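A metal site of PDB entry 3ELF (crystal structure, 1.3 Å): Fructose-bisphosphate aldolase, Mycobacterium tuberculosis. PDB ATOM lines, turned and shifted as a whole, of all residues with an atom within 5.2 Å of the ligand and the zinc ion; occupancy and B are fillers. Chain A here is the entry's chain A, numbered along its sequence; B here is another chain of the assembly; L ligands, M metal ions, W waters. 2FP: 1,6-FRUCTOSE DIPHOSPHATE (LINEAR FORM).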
ATOM      1  N   ASN A  27       9.961   8.333  10.535  1.00  0.00           N
ATOM      2  CA  ASN A  27       9.683   7.628   9.297  1.00  0.00           C
ATOM      3  C   ASN A  27      10.967   7.370   8.523  1.00  0.00           C
ATOM      4  O   ASN A  27      11.789   8.272   8.321  1.00  0.00           O
ATOM      5  CB  ASN A  27       8.713   8.398   8.417  1.00  0.00           C
ATOM      6  CG  ASN A  27       7.300   8.327   8.920  1.00  0.00           C
ATOM      7  OD1 ASN A  27       6.907   9.077   9.815  1.00  0.00           O
ATOM      8  ND2 ASN A  27       6.504   7.414   8.355  1.00  0.00           N
ATOM      9  N   GLN A  51       9.543   3.910  11.986  1.00  0.00           N
ATOM     10  CA  GLN A  51       8.271   3.567  11.361  1.00  0.00           C
ATOM     11  C   GLN A  51       8.292   3.603   9.841  1.00  0.00           C
ATOM     12  O   GLN A  51       9.014   4.415   9.243  1.00  0.00           O
ATOM     13  CB  GLN A  51       7.099   4.369  11.930  1.00  0.00           C
ATOM     14  CG  GLN A  51       7.185   5.876  11.802  1.00  0.00           C
ATOM     15  CD  GLN A  51       6.017   6.574  12.484  1.00  0.00           C
ATOM     16  OE1 GLN A  51       5.490   6.088  13.491  1.00  0.00           O
ATOM     17  NE2 GLN A  51       5.613   7.720  11.938  1.00  0.00           N
ATOM     18  N   SER A  53       5.700   3.958   6.605  1.00  0.00           N
ATOM     19  CA  SER A  53       4.390   4.206   6.025  1.00  0.00           C
ATOM     20  C   SER A  53       4.124   3.205   4.902  1.00  0.00           C
ATOM     21  O   SER A  53       5.015   2.474   4.486  1.00  0.00           O
ATOM     22  CB  SER A  53       4.346   5.627   5.472  1.00  0.00           C
ATOM     23  OG  SER A  53       5.240   5.737   4.393  1.00  0.00           O
ATOM     24  N   GLY A  55       3.591   3.983   1.809  1.00  0.00           N
ATOM     25  CA  GLY A  55       4.438   4.449   0.702  1.00  0.00           C
ATOM     26  C   GLY A  55       5.913   4.193   0.955  1.00  0.00           C
ATOM     27  O   GLY A  55       6.671   3.897   0.027  1.00  0.00           O
ATOM     28  N   GLY A  56       6.348   4.330   2.197  1.00  0.00           N
ATOM     29  CA  GLY A  56       7.730   4.038   2.548  1.00  0.00           C
ATOM     30  C   GLY A  56       8.048   2.570   2.334  1.00  0.00           C
ATOM     31  O   GLY A  56       9.110   2.226   1.810  1.00  0.00           O
ATOM     32  N   ASP A  95       3.053   2.797   9.958  1.00  0.00           N
ATOM     33  CA  ASP A  95       2.286   4.042  10.015  1.00  0.00           C
ATOM     34  C   ASP A  95       0.953   3.890   9.248  1.00  0.00           C
ATOM     35  O   ASP A  95       0.628   2.801   8.742  1.00  0.00           O
ATOM     36  CB  ASP A  95       3.159   5.164   9.445  1.00  0.00           C
ATOM     37  CG  ASP A  95       2.767   6.548   9.948  1.00  0.00           C
ATOM     38  OD1 ASP A  95       1.852   6.694  10.778  1.00  0.00           O
ATOM     39  OD2 ASP A  95       3.426   7.504   9.462  1.00  0.00           O
ATOM     40  N   HIS A  96       0.175   4.978   9.185  1.00  0.00           N
ATOM     41  CA  HIS A  96      -1.190   5.019   8.620  1.00  0.00           C
ATOM     42  C   HIS A  96      -1.589   3.876   7.687  1.00  0.00           C
ATOM     43  O   HIS A  96      -1.127   3.806   6.549  1.00  0.00           O
ATOM     44  CB  HIS A  96      -1.428   6.324   7.840  1.00  0.00           C
ATOM     45  CG  HIS A  96      -1.228   7.570   8.648  1.00  0.00           C
ATOM     46  ND1 HIS A  96      -2.234   8.167   9.372  1.00  0.00           N
ATOM     47  CD2 HIS A  96      -0.127   8.347   8.816  1.00  0.00           C
ATOM     48  CE1 HIS A  96      -1.759   9.253   9.959  1.00  0.00           C
ATOM     49  NE2 HIS A  96      -0.493   9.392   9.631  1.00  0.00           N
ATOM     50  N   VAL A 211      -0.806  19.074  12.028  1.00  0.00           N
ATOM     51  CA  VAL A 211      -0.779  19.027  10.571  1.00  0.00           C
ATOM     52  C   VAL A 211       0.494  18.333  10.081  1.00  0.00           C
ATOM     53  O   VAL A 211       1.594  18.684  10.535  1.00  0.00           O
ATOM     54  CB  VAL A 211      -0.857  20.467   9.950  1.00  0.00           C
ATOM     55  CG1 VAL A 211      -0.794  20.423   8.421  1.00  0.00           C
ATOM     56  CG2 VAL A 211      -2.122  21.196  10.398  1.00  0.00           C
ATOM     57  N   HIS A 212       0.358  17.382   9.163  1.00  0.00           N
ATOM     58  CA  HIS A 212       1.513  16.773   8.499  1.00  0.00           C
ATOM     59  C   HIS A 212       2.153  17.807   7.577  1.00  0.00           C
ATOM     60  O   HIS A 212       1.439  18.495   6.841  1.00  0.00           O
ATOM     61  CB  HIS A 212       1.072  15.590   7.630  1.00  0.00           C
ATOM     62  CG  HIS A 212       0.582  14.401   8.403  1.00  0.00           C
ATOM     63  ND1 HIS A 212      -0.659  13.860   8.202  1.00  0.00           N
ATOM     64  CD2 HIS A 212       1.189  13.626   9.337  1.00  0.00           C
ATOM     65  CE1 HIS A 212      -0.815  12.802   8.986  1.00  0.00           C
ATOM     66  NE2 HIS A 212       0.299  12.636   9.682  1.00  0.00           N
ATOM     67  N   GLY A 213       3.481  17.876   7.602  1.00  0.00           N
ATOM     68  CA  GLY A 213       4.210  18.816   6.756  1.00  0.00           C
ATOM     69  C   GLY A 213       4.835  19.940   7.553  1.00  0.00           C
ATOM     70  O   GLY A 213       4.647  20.039   8.768  1.00  0.00           O
ATOM     71  N   VAL A 214       5.582  20.791   6.857  1.00  0.00           N
ATOM     72  CA  VAL A 214       6.271  21.921   7.481  1.00  0.00           C
ATOM     73  C   VAL A 214       5.890  23.216   6.785  1.00  0.00           C
ATOM     74  O   VAL A 214       6.126  23.374   5.586  1.00  0.00           O
ATOM     75  CB  VAL A 214       7.806  21.732   7.473  1.00  0.00           C
ATOM     76  CG1 VAL A 214       8.529  23.023   7.881  1.00  0.00           C
ATOM     77  CG2 VAL A 214       8.186  20.605   8.401  1.00  0.00           C
ATOM     78  N   PHE A 251       1.397  12.049  18.691  1.00  0.00           N
ATOM     79  CA  PHE A 251       1.404  13.380  18.089  1.00  0.00           C
ATOM     80  C   PHE A 251       1.889  13.226  16.643  1.00  0.00           C
ATOM     81  O   PHE A 251       3.100  13.146  16.401  1.00  0.00           O
ATOM     82  CB  PHE A 251       2.336  14.247  18.942  1.00  0.00           C
ATOM     83  CG  PHE A 251       2.474  15.703  18.515  1.00  0.00           C
ATOM     84  CD1 PHE A 251       2.063  16.185  17.282  1.00  0.00           C
ATOM     85  CD2 PHE A 251       3.100  16.588  19.399  1.00  0.00           C
ATOM     86  CE1 PHE A 251       2.269  17.529  16.930  1.00  0.00           C
ATOM     87  CE2 PHE A 251       3.298  17.919  19.064  1.00  0.00           C
ATOM     88  CZ  PHE A 251       2.876  18.392  17.831  1.00  0.00           C
ATOM     89  N   HIS A 252       0.951  13.132  15.708  1.00  0.00           N
ATOM     90  CA  HIS A 252       1.284  13.131  14.284  1.00  0.00           C
ATOM     91  C   HIS A 252       1.599  14.547  13.821  1.00  0.00           C
ATOM     92  O   HIS A 252       1.074  15.512  14.357  1.00  0.00           O
ATOM     93  CB  HIS A 252       0.132  12.580  13.462  1.00  0.00           C
ATOM     94  CG  HIS A 252       0.025  11.087  13.495  1.00  0.00           C
ATOM     95  ND1 HIS A 252       0.291  10.305  12.386  1.00  0.00           N
ATOM     96  CD2 HIS A 252      -0.273  10.241  14.501  1.00  0.00           C
ATOM     97  CE1 HIS A 252       0.149   9.038  12.715  1.00  0.00           C
ATOM     98  NE2 HIS A 252      -0.186   8.959  13.993  1.00  0.00           N
ATOM     99  N   GLY A 253       2.423  14.661  12.792  1.00  0.00           N
ATOM    100  CA  GLY A 253       2.733  15.977  12.257  1.00  0.00           C
ATOM    101  C   GLY A 253       3.697  16.764  13.122  1.00  0.00           C
ATOM    102  O   GLY A 253       3.627  17.995  13.173  1.00  0.00           O
ATOM    103  N   GLY A 254       4.634  16.082  13.770  1.00  0.00           N
ATOM    104  CA  GLY A 254       5.562  16.726  14.698  1.00  0.00           C
ATOM    105  C   GLY A 254       6.522  17.729  14.078  1.00  0.00           C
ATOM    106  O   GLY A 254       6.921  18.686  14.738  1.00  0.00           O
ATOM    107  N   SER A 255       6.905  17.537  12.817  1.00  0.00           N
ATOM    108  CA  SER A 255       7.875  18.432  12.187  1.00  0.00           C
ATOM    109  C   SER A 255       7.379  19.862  12.178  1.00  0.00           C
ATOM    110  O   SER A 255       6.186  20.106  11.967  1.00  0.00           O
ATOM    111  CB  SER A 255       8.176  18.005  10.752  1.00  0.00           C
ATOM    112  OG  SER A 255       8.763  16.719  10.701  1.00  0.00           O
ATOM    113  N   ASN A 274       5.553  11.676  15.992  1.00  0.00           N
ATOM    114  CA  ASN A 274       5.976  11.269  14.672  1.00  0.00           C
ATOM    115  C   ASN A 274       6.679  12.418  13.971  1.00  0.00           C
ATOM    116  O   ASN A 274       6.190  13.549  13.974  1.00  0.00           O
ATOM    117  CB  ASN A 274       4.783  10.873  13.803  1.00  0.00           C
ATOM    118  CG  ASN A 274       4.047   9.618  14.268  1.00  0.00           C
ATOM    119  OD1 ASN A 274       3.169   9.115  13.563  1.00  0.00           O
ATOM    120  ND2 ASN A 274       4.404   9.092  15.434  1.00  0.00           N
ATOM    121  N   VAL A 275       7.827  12.106  13.360  1.00  0.00           N
ATOM    122  CA  VAL A 275       8.619  13.069  12.610  1.00  0.00           C
ATOM    123  C   VAL A 275       8.968  12.435  11.256  1.00  0.00           C
ATOM    124  O   VAL A 275       9.466  11.294  11.189  1.00  0.00           O
ATOM    125  CB  VAL A 275       9.904  13.448  13.386  1.00  0.00           C
ATOM    126  CG1 VAL A 275      10.840  14.300  12.535  1.00  0.00           C
ATOM    127  CG2 VAL A 275       9.550  14.196  14.671  1.00  0.00           C
ATOM    128  N   ASP A 276       8.694  13.153  10.175  1.00  0.00           N
ATOM    129  CA  ASP A 276       9.131  12.729   8.849  1.00  0.00           C
ATOM    130  C   ASP A 276       9.697  13.907   8.083  1.00  0.00           C
ATOM    131  O   ASP A 276      10.848  13.878   7.666  1.00  0.00           O
ATOM    132  CB  ASP A 276       7.973  12.076   8.069  1.00  0.00           C
ATOM    133  CG  ASP A 276       8.447  11.262   6.860  1.00  0.00           C
ATOM    134  OD1 ASP A 276       9.664  11.207   6.581  1.00  0.00           O
ATOM    135  OD2 ASP A 276       7.573  10.635   6.204  1.00  0.00           O
ATOM    136  N   THR A 277       8.908  14.957   7.911  1.00  0.00           N
ATOM    137  CA  THR A 277       9.310  16.047   7.035  1.00  0.00           C
ATOM    138  C   THR A 277      10.652  16.682   7.450  1.00  0.00           C
ATOM    139  O   THR A 277      11.517  16.928   6.596  1.00  0.00           O
ATOM    140  CB  THR A 277       8.185  17.092   6.929  1.00  0.00           C
ATOM    141  OG1 THR A 277       6.986  16.456   6.475  1.00  0.00           O
ATOM    142  CG2 THR A 277       8.545  18.169   5.937  1.00  0.00           C
ATOM    143  N   ASP A 278      10.845  16.933   8.740  1.00  0.00           N
ATOM    144  CA  ASP A 278      12.079  17.561   9.192  1.00  0.00           C
ATOM    145  C   ASP A 278      13.306  16.663   9.013  1.00  0.00           C
ATOM    146  O   ASP A 278      14.391  17.160   8.726  1.00  0.00           O
ATOM    147  CB  ASP A 278      11.962  18.035  10.635  1.00  0.00           C
ATOM    148  CG  ASP A 278      11.319  19.415  10.767  1.00  0.00           C
ATOM    149  OD1 ASP A 278      11.105  20.106   9.746  1.00  0.00           O
ATOM    150  OD2 ASP A 278      11.014  19.799  11.921  1.00  0.00           O
ATOM    151  N   LYS B 308       8.452  20.130   0.409  1.00  0.00           N
ATOM    152  CA  LYS B 308       8.565  18.750   0.886  1.00  0.00           C
ATOM    153  C   LYS B 308       8.545  17.725  -0.233  1.00  0.00           C
ATOM    154  O   LYS B 308       9.308  16.752  -0.194  1.00  0.00           O
ATOM    155  CB  LYS B 308       7.452  18.451   1.883  1.00  0.00           C
ATOM    156  CG  LYS B 308       7.318  16.980   2.282  1.00  0.00           C
ATOM    157  CD  LYS B 308       6.064  16.771   3.127  1.00  0.00           C
ATOM    158  CE  LYS B 308       5.803  15.288   3.377  1.00  0.00           C
ATOM    159  NZ  LYS B 308       6.832  14.709   4.280  1.00  0.00           N
ATOM    160  N   ASP B 312      11.678  15.224  -0.029  1.00  0.00           N
ATOM    161  CA  ASP B 312      11.405  13.828   0.305  1.00  0.00           C
ATOM    162  C   ASP B 312      12.444  12.967  -0.440  1.00  0.00           C
ATOM    163  O   ASP B 312      12.505  13.026  -1.661  1.00  0.00           O
ATOM    164  CB  ASP B 312       9.991  13.493  -0.171  1.00  0.00           C
ATOM    165  CG  ASP B 312       9.550  12.074   0.164  1.00  0.00           C
ATOM    166  OD1 ASP B 312       8.330  11.898   0.360  1.00  0.00           O
ATOM    167  OD2 ASP B 312      10.384  11.148   0.213  1.00  0.00           O
ATOM    168  N   ARG B 314      12.632   9.999  -1.354  1.00  0.00           N
ATOM    169  CA  ARG B 314      12.070   9.108  -2.366  1.00  0.00           C
ATOM    170  C   ARG B 314      11.924   9.775  -3.718  1.00  0.00           C
ATOM    171  O   ARG B 314      11.987   9.104  -4.744  1.00  0.00           O
ATOM    172  CB  ARG B 314      10.736   8.528  -1.908  1.00  0.00           C
ATOM    173  CG  ARG B 314      10.864   7.693  -0.659  1.00  0.00           C
ATOM    174  CD  ARG B 314       9.503   7.357  -0.102  1.00  0.00           C
ATOM    175  NE  ARG B 314       8.865   8.547   0.461  1.00  0.00           N
ATOM    176  CZ  ARG B 314       7.732   8.539   1.138  1.00  0.00           C
ATOM    177  NH1 ARG B 314       7.075   7.404   1.321  1.00  0.00           N
ATOM    178  NH2 ARG B 314       7.240   9.682   1.614  1.00  0.00           N
HETATM  179  P6  2FP L   1       4.248   9.101   3.637  1.00  0.00           P
HETATM  180  O6  2FP L   1       4.492   9.406   5.202  1.00  0.00           O
HETATM  181  C6  2FP L   1       3.568  10.155   5.996  1.00  0.00           C
HETATM  182  C5  2FP L   1       4.142  10.256   7.409  1.00  0.00           C
HETATM  183  O5  2FP L   1       5.337  11.039   7.344  1.00  0.00           O
HETATM  184  C4  2FP L   1       3.254  10.980   8.401  1.00  0.00           C
HETATM  185  O4  2FP L   1       1.864  10.619   8.258  1.00  0.00           O
HETATM  186  C3  2FP L   1       3.731  10.697   9.820  1.00  0.00           C
HETATM  187  O3  2FP L   1       2.793   9.798  10.455  1.00  0.00           O
HETATM  188  C2  2FP L   1       3.784  11.995  10.582  1.00  0.00           C
HETATM  189  O2  2FP L   1       2.899  12.204  11.392  1.00  0.00           O
HETATM  190  C1  2FP L   1       4.908  13.013  10.369  1.00  0.00           C
HETATM  191  O1  2FP L   1       4.459  14.385  10.139  1.00  0.00           O
HETATM  192  O61 2FP L   1       2.810   8.633   3.556  1.00  0.00           O
HETATM  193  O62 2FP L   1       4.528  10.402   2.918  1.00  0.00           O
HETATM  194  O63 2FP L   1       5.272   8.042   3.342  1.00  0.00           O
HETATM  195  P1  2FP L   1       5.522  15.564   9.788  1.00  0.00           P
HETATM  196  O11 2FP L   1       5.935  15.234   8.368  1.00  0.00           O
HETATM  197  O12 2FP L   1       6.654  15.285  10.749  1.00  0.00           O
HETATM  198  O13 2FP L   1       4.848  16.901  10.031  1.00  0.00           O
HETATM  199 ZN    ZN M   1       0.884  10.794  10.422  1.00  0.00          ZN
HETATM  200  O   HOH W   1       2.234   6.376   2.337  1.00  0.00           O
HETATM  201  O   HOH W   2       4.812  13.706   6.591  1.00  0.00           O
HETATM  202  O   HOH W   3       7.751   8.141   4.820  1.00  0.00           O
HETATM  203  O   HOH W   4       3.067  12.604   2.600  1.00  0.00           O
HETATM  204  O   HOH W   5       0.638   9.972   2.767  1.00  0.00           O
HETATM  205  O   HOH W   6       1.167   7.615   5.540  1.00  0.00           O
HETATM  206  O   HOH W   7       0.868  12.009   6.192  1.00  0.00           O
HETATM  207  O   HOH W   8       4.028  10.165   0.162  1.00  0.00           O
HETATM  208  O   HOH W   9       6.543  11.929   3.921  1.00  0.00           O
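The backbone NH of Thr 277 is in hydrogen-bond range of an oxygen (O11) of the ligand (3.0 Å).
OG1 of Thr 277 is in hydrogen-bond range of O11 of the ligand (2.5 Å).
OG of Ser 53 lies within hydrogen-bond range of O63 of the ligand, 2.5 Å away.
An oxygen (O12) of the ligand sits at hydrogen-bond distance from the backbone NH of Asp 276 (3.0 Å).
OD2 of Asp 276 sits at hydrogen-bond distance from O5 of the ligand, 2.5 Å away.
N of Ser 255 sits at hydrogen-bond distance from O12 of the ligand (3.1 Å).
OG of Ser 255 is in hydrogen-bond range of O12 of the ligand (2.6 Å).
OD2 of Asp 95 sits close to O3 of the ligand (2.6 Å).
The guanidinium group (NH1) of Arg 314 of chain B lies within salt-bridge range of an oxygen (O63) of the ligand, 2.8 Å away.
The backbone NH of Gly 253 is in hydrogen-bond range of an oxygen (O2) of the ligand, at 2.9 Å.
N of Gly 213 sits at hydrogen-bond distance from O13 of the ligand (3.0 Å).
The side-chain amide oxygen of Asn 274 lies close to an oxygen (O3) of the ligand (3.2 Å).
Asn 27 touches the ligand (OD1 to O5, 3.5 Å).
Gln 51 touches the ligand.
Val 211 touches the ligand.
Gly 254 touches the ligand (N to O12, 3.7 Å).
CA of Val 275 touches O12 of the ligand, at 3.5 Å.
Hydrophobic or aromatic side chains within 4 Å of the ligand: His 96, His 212 and His 252.
Within 4 Å of the ligand: Asn 27, Gln 51, Ser 53, Asp 95, His 96, Val 211, His 212, Gly 213, His 252, Gly 253, Gly 254, Ser 255, Asn 274, Val 275, Asp 276, Thr 277 and Arg 314 of chain B.
The zinc ion is bound by NE2 of His 212 (2.1 Å), ND1 of His 252 (2.1 Å), NE2 of His 96 (2.1 Å), O3 of the ligand (2.2 Å) and O4 of the ligand (2.4 Å).
The zinc ion has five donor atoms within binding distance.
Slightly farther from the zinc ion lies an oxygen (O2) of the ligand (2.6 Å).
Within 4 Å of the zinc ion: His 96, His 212 and His 252.
Along chain A the residues within 4 Å of the zinc ion span positions 96 to 252.
The nearest printed residue that does not touch the zinc ion is Asp 95 (4.2 Å).
The side-chain amide oxygen (OD1) of Asn 274 lies close to a ring nitrogen (NE2) of His 252, 3.4 Å away.
The side-chain hydroxyl (OG1) of Thr 277 lies within hydrogen-bond range of the side-chain amino group (NZ) of Lys 308 of chain B (2.8 Å).
The side-chain hydroxyl (OG) of Ser 53 lies within hydrogen-bond range of the backbone NH (N) of Gly 56.
The side-chain hydroxyl of Ser 255 lies within hydrogen-bond range of the backbone NH of Asp 278 (2.9 Å).
The side-chain carboxylate of Asp 95 is in hydrogen-bond range of the side-chain amide nitrogen of Gln 51 (3.3 Å).
The guanidinium group (NH2) of Arg 314 of chain B is in salt-bridge range of the side-chain carboxylate (OD1) of Asp 312 of chain B (2.8 Å).
The backbone carbonyl oxygen (O) of Asn 274 is in hydrogen-bond range of the backbone NH (N) of Gly 254 (3.0 Å).
The side-chain amide oxygen (OD1) of Asn 274 sits at hydrogen-bond distance from the side-chain amide nitrogen (NE2) of Gln 51, at 3.2 Å.
Water W2 lies within hydrogen-bond range of an oxygen (O11) of the ligand (2.6 Å) and the side-chain amino group of Lys 308 of chain B (3.2 Å).
Water W1 lies within hydrogen-bond range of O61 of the ligand (2.6 Å) and N of Gly 55 (2.8 Å).
Water W9 lies within hydrogen-bond range of an oxygen (O62) of the ligand, the side-chain amino group of Lys 308 of chain B, the side-chain carboxylate of Asp 276 and the guanidinium group of Arg 314 of chain B.
Water W3 bridges the side-chain carboxylate (OD2) of Asp 276 (2.9 Å) and an oxygen (O63) of the ligand (2.9 Å).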
